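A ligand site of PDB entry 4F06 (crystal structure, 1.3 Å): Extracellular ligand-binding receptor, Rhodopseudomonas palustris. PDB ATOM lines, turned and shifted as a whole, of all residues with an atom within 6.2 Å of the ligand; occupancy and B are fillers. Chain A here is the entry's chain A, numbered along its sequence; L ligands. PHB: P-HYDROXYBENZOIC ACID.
OG1 of Thr 106 sits at hydrogen-bond distance from OG1 of Thr 82, 2.8 Å away.
The side-chain carboxylate (OD1) of Asp 232 lies within hydrogen-bond range of the side-chain hydroxyl (OH) of Tyr 253, at 2.8 Å.
O of Ala 105 is in hydrogen-bond range of N of Met 123.
OH of Tyr 80 sits at hydrogen-bond distance from O of Ala 204, at 2.7 Å.
The backbone NH (N) of Ala 104 is in hydrogen-bond range of the backbone carbonyl oxygen (O) of Tyr 80 (3.5 Å).
The side-chain amide nitrogen of Asn 103 lies within hydrogen-bond range of the backbone carbonyl oxygen of Tyr 80 (2.9 Å).
The backbone NH of Thr 82 sits at hydrogen-bond distance from an oxygen (O2') of the ligand, at 2.8 Å.
An oxygen (O1') of the ligand sits at hydrogen-bond distance from the side-chain hydroxyl (OG1) of Thr 82 (2.6 Å).
The side-chain carboxylate (OD1) of Asp 232 lies within hydrogen-bond range of an oxygen (O4) of the ligand, 2.7 Å away.
OH of Tyr 149 is in hydrogen-bond range of O2' of the ligand, 2.7 Å away.
N of Ala 105 lies within hydrogen-bond range of O1' of the ligand (3.0 Å).
The backbone NH (N) of Ala 204 lies within hydrogen-bond range of an oxygen (O4) of the ligand (3.1 Å).
Tyr 80 touches the ligand.
Phe 81 touches the ligand.
Asn 103 touches the ligand.
Ala 104 touches the ligand (CA to O1', 3.4 Å).
Phe 121 touches the ligand.
Pro 151 touches the ligand.
CE1 of Phe 201 touches C3 of the ligand (3.6 Å).
Pro 203 touches the ligand (CB to C5, 3.5 Å).
Met 283 touches the ligand.
Hydrophobic or aromatic side chains that line the ligand: Tyr 80, Phe 81, Ala 105, Phe 121, Tyr 149, Pro 151, Phe 201, Pro 203, Ala 204 and Met 283.
Of the 20 residues printed, 14 come within 4 Å of the ligand.
The nearest printed residue that does not touch the ligand is Thr 106 (4.3 Å).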
ATOM      1  N   TYR A  80      -2.590 -10.741  11.102  1.00  0.00           N
ATOM      2  CA  TYR A  80      -2.911 -11.411  12.350  1.00  0.00           C
ATOM      3  C   TYR A  80      -3.694 -12.728  12.107  1.00  0.00           C
ATOM      4  O   TYR A  80      -3.351 -13.778  12.663  1.00  0.00           O
ATOM      5  CB  TYR A  80      -3.722 -10.471  13.254  1.00  0.00           C
ATOM      6  CG  TYR A  80      -3.841 -10.968  14.668  1.00  0.00           C
ATOM      7  CD1 TYR A  80      -2.696 -11.126  15.457  1.00  0.00           C
ATOM      8  CD2 TYR A  80      -5.092 -11.299  15.224  1.00  0.00           C
ATOM      9  CE1 TYR A  80      -2.792 -11.608  16.763  1.00  0.00           C
ATOM     10  CE2 TYR A  80      -5.221 -11.743  16.550  1.00  0.00           C
ATOM     11  CZ  TYR A  80      -4.055 -11.907  17.303  1.00  0.00           C
ATOM     12  OH  TYR A  80      -4.084 -12.392  18.598  1.00  0.00           O
ATOM     13  N   PHE A  81      -4.764 -12.647  11.286  1.00  0.00           N
ATOM     14  CA  PHE A  81      -5.644 -13.790  11.115  1.00  0.00           C
ATOM     15  C   PHE A  81      -5.323 -14.629   9.868  1.00  0.00           C
ATOM     16  O   PHE A  81      -5.136 -14.066   8.771  1.00  0.00           O
ATOM     17  CB  PHE A  81      -7.108 -13.311  11.039  1.00  0.00           C
ATOM     18  CG  PHE A  81      -7.645 -12.736  12.346  1.00  0.00           C
ATOM     19  CD1 PHE A  81      -7.884 -13.599  13.409  1.00  0.00           C
ATOM     20  CD2 PHE A  81      -7.913 -11.384  12.487  1.00  0.00           C
ATOM     21  CE1 PHE A  81      -8.388 -13.122  14.610  1.00  0.00           C
ATOM     22  CE2 PHE A  81      -8.423 -10.903  13.694  1.00  0.00           C
ATOM     23  CZ  PHE A  81      -8.672 -11.775  14.754  1.00  0.00           C
ATOM     24  N   THR A  82      -5.410 -15.919  10.060  1.00  0.00           N
ATOM     25  CA  THR A  82      -5.215 -16.846   8.927  1.00  0.00           C
ATOM     26  C   THR A  82      -6.041 -16.495   7.673  1.00  0.00           C
ATOM     27  O   THR A  82      -5.479 -16.447   6.603  1.00  0.00           O
ATOM     28  CB  THR A  82      -5.454 -18.290   9.386  1.00  0.00           C
ATOM     29  OG1 THR A  82      -4.337 -18.764  10.115  1.00  0.00           O
ATOM     30  CG2 THR A  82      -5.682 -19.250   8.212  1.00  0.00           C
ATOM     31  N   PRO A  83      -7.377 -16.306   7.779  1.00  0.00           N
ATOM     32  CA  PRO A  83      -8.157 -16.045   6.563  1.00  0.00           C
ATOM     33  C   PRO A  83      -7.725 -14.800   5.835  1.00  0.00           C
ATOM     34  O   PRO A  83      -7.885 -14.687   4.630  1.00  0.00           O
ATOM     35  CB  PRO A  83      -9.625 -15.973   7.072  1.00  0.00           C
ATOM     36  CG  PRO A  83      -9.505 -15.794   8.577  1.00  0.00           C
ATOM     37  CD  PRO A  83      -8.261 -16.577   8.932  1.00  0.00           C
ATOM     38  N   ASN A 103       2.092 -13.196  12.153  1.00  0.00           N
ATOM     39  CA  ASN A 103       1.296 -13.929  13.142  1.00  0.00           C
ATOM     40  C   ASN A 103       0.618 -15.161  12.537  1.00  0.00           C
ATOM     41  O   ASN A 103       0.885 -16.303  12.969  1.00  0.00           O
ATOM     42  CB  ASN A 103       0.235 -13.075  13.871  1.00  0.00           C
ATOM     43  CG  ASN A 103      -0.348 -13.843  15.029  1.00  0.00           C
ATOM     44  OD1 ASN A 103       0.327 -14.033  16.051  1.00  0.00           O
ATOM     45  ND2 ASN A 103      -1.575 -14.344  14.888  1.00  0.00           N
ATOM     46  N   ALA A 104      -0.289 -14.949  11.565  1.00  0.00           N
ATOM     47  CA  ALA A 104      -1.198 -16.027  11.082  1.00  0.00           C
ATOM     48  C   ALA A 104      -0.449 -17.346  11.008  1.00  0.00           C
ATOM     49  O   ALA A 104       0.587 -17.469  10.324  1.00  0.00           O
ATOM     50  CB  ALA A 104      -1.688 -15.631   9.715  1.00  0.00           C
ATOM     51  N   ALA A 105      -1.003 -18.390  11.662  1.00  0.00           N
ATOM     52  CA  ALA A 105      -0.191 -19.509  12.153  1.00  0.00           C
ATOM     53  C   ALA A 105      -0.636 -20.855  11.525  1.00  0.00           C
ATOM     54  O   ALA A 105      -0.168 -21.922  11.938  1.00  0.00           O
ATOM     55  CB  ALA A 105      -0.287 -19.578  13.662  1.00  0.00           C
ATOM     56  N   THR A 106      -1.547 -20.852  10.540  1.00  0.00           N
ATOM     57  CA  THR A 106      -1.992 -22.122   9.911  1.00  0.00           C
ATOM     58  C   THR A 106      -0.829 -22.609   9.025  1.00  0.00           C
ATOM     59  O   THR A 106      -0.239 -21.850   8.231  1.00  0.00           O
ATOM     60  CB  THR A 106      -3.288 -21.879   9.135  1.00  0.00           C
ATOM     61  OG1 THR A 106      -4.297 -21.534  10.107  1.00  0.00           O
ATOM     62  CG2 THR A 106      -3.762 -23.118   8.366  1.00  0.00           C
ATOM     63  N   ILE A 109      -0.318 -21.866   5.074  1.00  0.00           N
ATOM     64  CA  ILE A 109      -0.190 -20.510   4.499  1.00  0.00           C
ATOM     65  C   ILE A 109       1.077 -20.427   3.654  1.00  0.00           C
ATOM     66  O   ILE A 109       1.063 -19.814   2.589  1.00  0.00           O
ATOM     67  CB  ILE A 109      -0.193 -19.465   5.609  1.00  0.00           C
ATOM     68  CG1 ILE A 109      -1.577 -19.392   6.275  1.00  0.00           C
ATOM     69  CG2 ILE A 109       0.233 -18.097   5.059  1.00  0.00           C
ATOM     70  CD1 ILE A 109      -1.626 -18.509   7.517  1.00  0.00           C
ATOM     71  N   PHE A 121       4.952 -18.400  14.021  1.00  0.00           N
ATOM     72  CA  PHE A 121       4.873 -19.767  14.575  1.00  0.00           C
ATOM     73  C   PHE A 121       3.831 -20.469  13.760  1.00  0.00           C
ATOM     74  O   PHE A 121       3.059 -19.832  13.024  1.00  0.00           O
ATOM     75  CB  PHE A 121       4.491 -19.755  16.090  1.00  0.00           C
ATOM     76  CG  PHE A 121       3.186 -19.003  16.383  1.00  0.00           C
ATOM     77  CD1 PHE A 121       3.234 -17.591  16.474  1.00  0.00           C
ATOM     78  CD2 PHE A 121       1.975 -19.659  16.567  1.00  0.00           C
ATOM     79  CE1 PHE A 121       2.067 -16.866  16.782  1.00  0.00           C
ATOM     80  CE2 PHE A 121       0.801 -18.939  16.854  1.00  0.00           C
ATOM     81  CZ  PHE A 121       0.862 -17.557  16.932  1.00  0.00           C
ATOM     82  N   MET A 123       0.596 -23.527  14.442  1.00  0.00           N
ATOM     83  CA  MET A 123      -0.138 -24.246  15.468  1.00  0.00           C
ATOM     84  C   MET A 123       0.439 -25.631  15.711  1.00  0.00           C
ATOM     85  O   MET A 123       0.607 -26.045  16.834  1.00  0.00           O
ATOM     86  CB  MET A 123      -1.609 -24.337  15.095  1.00  0.00           C
ATOM     87  CG  MET A 123      -2.263 -22.957  14.902  1.00  0.00           C
ATOM     88  SD  MET A 123      -2.043 -21.740  16.400  1.00  0.00           S
ATOM     89  CE  MET A 123      -2.684 -22.913  17.782  1.00  0.00           C
ATOM     90  N   TYR A 149     -11.887 -22.455  13.054  1.00  0.00           N
ATOM     91  CA  TYR A 149     -11.352 -21.957  11.787  1.00  0.00           C
ATOM     92  C   TYR A 149      -9.922 -22.501  11.655  1.00  0.00           C
ATOM     93  O   TYR A 149      -9.457 -23.232  12.516  1.00  0.00           O
ATOM     94  CB  TYR A 149     -11.430 -20.404  11.637  1.00  0.00           C
ATOM     95  CG  TYR A 149     -10.406 -19.590  12.442  1.00  0.00           C
ATOM     96  CD1 TYR A 149     -10.216 -19.754  13.831  1.00  0.00           C
ATOM     97  CD2 TYR A 149      -9.689 -18.591  11.807  1.00  0.00           C
ATOM     98  CE1 TYR A 149      -9.278 -18.974  14.510  1.00  0.00           C
ATOM     99  CE2 TYR A 149      -8.752 -17.811  12.487  1.00  0.00           C
ATOM    100  CZ  TYR A 149      -8.552 -18.022  13.837  1.00  0.00           C
ATOM    101  OH  TYR A 149      -7.637 -17.265  14.524  1.00  0.00           O
ATOM    102  N   PRO A 151      -6.553 -22.210  12.125  1.00  0.00           N
ATOM    103  CA  PRO A 151      -5.496 -22.565  13.072  1.00  0.00           C
ATOM    104  C   PRO A 151      -6.061 -23.444  14.210  1.00  0.00           C
ATOM    105  O   PRO A 151      -5.322 -24.258  14.763  1.00  0.00           O
ATOM    106  CB  PRO A 151      -4.996 -21.199  13.574  1.00  0.00           C
ATOM    107  CG  PRO A 151      -6.158 -20.276  13.366  1.00  0.00           C
ATOM    108  CD  PRO A 151      -6.797 -20.751  12.071  1.00  0.00           C
ATOM    109  N   PHE A 201      -7.068 -23.882  22.090  1.00  0.00           N
ATOM    110  CA  PHE A 201      -6.596 -22.726  21.363  1.00  0.00           C
ATOM    111  C   PHE A 201      -7.795 -21.846  20.978  1.00  0.00           C
ATOM    112  O   PHE A 201      -8.807 -22.390  20.492  1.00  0.00           O
ATOM    113  CB  PHE A 201      -5.927 -23.112  20.024  1.00  0.00           C
ATOM    114  CG  PHE A 201      -5.838 -21.953  19.059  1.00  0.00           C
ATOM    115  CD1 PHE A 201      -4.875 -20.932  19.201  1.00  0.00           C
ATOM    116  CD2 PHE A 201      -6.787 -21.838  18.013  1.00  0.00           C
ATOM    117  CE1 PHE A 201      -4.852 -19.829  18.374  1.00  0.00           C
ATOM    118  CE2 PHE A 201      -6.751 -20.721  17.174  1.00  0.00           C
ATOM    119  CZ  PHE A 201      -5.797 -19.723  17.339  1.00  0.00           C
ATOM    120  N   LEU A 202      -7.665 -20.539  21.200  1.00  0.00           N
ATOM    121  CA  LEU A 202      -8.512 -19.528  20.572  1.00  0.00           C
ATOM    122  C   LEU A 202      -7.532 -18.410  20.198  1.00  0.00           C
ATOM    123  O   LEU A 202      -6.471 -18.278  20.818  1.00  0.00           O
ATOM    124  CB  LEU A 202      -9.584 -18.978  21.539  1.00  0.00           C
ATOM    125  CG  LEU A 202     -10.396 -20.004  22.342  1.00  0.00           C
ATOM    126  CD1 LEU A 202      -9.713 -20.379  23.655  1.00  0.00           C
ATOM    127  CD2 LEU A 202     -11.770 -19.429  22.631  1.00  0.00           C
ATOM    128  N   PRO A 203      -7.857 -17.546  19.239  1.00  0.00           N
ATOM    129  CA  PRO A 203      -6.933 -16.440  18.878  1.00  0.00           C
ATOM    130  C   PRO A 203      -6.810 -15.506  20.073  1.00  0.00           C
ATOM    131  O   PRO A 203      -7.805 -15.172  20.774  1.00  0.00           O
ATOM    132  CB  PRO A 203      -7.644 -15.749  17.710  1.00  0.00           C
ATOM    133  CG  PRO A 203      -9.092 -16.146  17.854  1.00  0.00           C
ATOM    134  CD  PRO A 203      -9.076 -17.563  18.409  1.00  0.00           C
ATOM    135  N   ALA A 204      -5.577 -15.068  20.335  1.00  0.00           N
ATOM    136  CA  ALA A 204      -5.342 -14.183  21.487  1.00  0.00           C
ATOM    137  C   ALA A 204      -6.159 -12.921  21.345  1.00  0.00           C
ATOM    138  O   ALA A 204      -6.242 -12.292  20.294  1.00  0.00           O
ATOM    139  CB  ALA A 204      -3.873 -13.865  21.565  1.00  0.00           C
ATOM    140  N   ASP A 232      -1.107 -18.609  22.920  1.00  0.00           N
ATOM    141  CA  ASP A 232      -2.140 -17.678  22.480  1.00  0.00           C
ATOM    142  C   ASP A 232      -3.135 -17.395  23.580  1.00  0.00           C
ATOM    143  O   ASP A 232      -3.760 -16.330  23.597  1.00  0.00           O
ATOM    144  CB  ASP A 232      -2.877 -18.316  21.299  1.00  0.00           C
ATOM    145  CG  ASP A 232      -1.896 -18.717  20.227  1.00  0.00           C
ATOM    146  OD1 ASP A 232      -1.476 -17.859  19.435  1.00  0.00           O
ATOM    147  OD2 ASP A 232      -1.487 -19.905  20.229  1.00  0.00           O
ATOM    148  N   TYR A 253       4.697 -22.388  23.974  1.00  0.00           N
ATOM    149  CA  TYR A 253       4.814 -21.275  23.065  1.00  0.00           C
ATOM    150  C   TYR A 253       6.253 -20.976  22.774  1.00  0.00           C
ATOM    151  O   TYR A 253       7.173 -21.315  23.561  1.00  0.00           O
ATOM    152  CB  TYR A 253       4.189 -20.004  23.640  1.00  0.00           C
ATOM    153  CG  TYR A 253       3.389 -19.118  22.693  1.00  0.00           C
ATOM    154  CD1 TYR A 253       2.545 -19.677  21.693  1.00  0.00           C
ATOM    155  CD2 TYR A 253       3.339 -17.725  22.869  1.00  0.00           C
ATOM    156  CE1 TYR A 253       1.705 -18.880  20.913  1.00  0.00           C
ATOM    157  CE2 TYR A 253       2.463 -16.921  22.142  1.00  0.00           C
ATOM    158  CZ  TYR A 253       1.654 -17.503  21.176  1.00  0.00           C
ATOM    159  OH  TYR A 253       0.807 -16.676  20.448  1.00  0.00           O
ATOM    160  N   MET A 283       3.538 -11.531  21.822  1.00  0.00           N
ATOM    161  CA  MET A 283       4.338 -12.272  20.845  1.00  0.00           C
ATOM    162  C   MET A 283       4.415 -11.618  19.475  1.00  0.00           C
ATOM    163  O   MET A 283       5.418 -11.829  18.752  1.00  0.00           O
ATOM    164  CB  MET A 283       3.754 -13.704  20.714  1.00  0.00           C
ATOM    165  CG  MET A 283       2.480 -13.833  19.854  1.00  0.00           C
ATOM    166  SD  MET A 283       0.907 -12.872  20.550  1.00  0.00           S
ATOM    167  CE  MET A 283      -0.431 -13.751  19.463  1.00  0.00           C
HETATM  168  C1' PHB L   1      -4.534 -17.061  13.182  1.00  0.00           C
HETATM  169  O1' PHB L   1      -3.764 -17.746  12.493  1.00  0.00           O
HETATM  170  O2' PHB L   1      -5.665 -16.647  12.738  1.00  0.00           O
HETATM  171  C1  PHB L   1      -4.137 -16.758  14.592  1.00  0.00           C
HETATM  172  C2  PHB L   1      -3.252 -17.613  15.267  1.00  0.00           C
HETATM  173  C3  PHB L   1      -2.921 -17.372  16.588  1.00  0.00           C
HETATM  174  C4  PHB L   1      -3.487 -16.308  17.258  1.00  0.00           C
HETATM  175  C5  PHB L   1      -4.354 -15.462  16.607  1.00  0.00           C
HETATM  176  C6  PHB L   1      -4.708 -15.686  15.282  1.00  0.00           C
HETATM  177  O4  PHB L   1      -3.233 -16.050  18.556  1.00  0.00           O
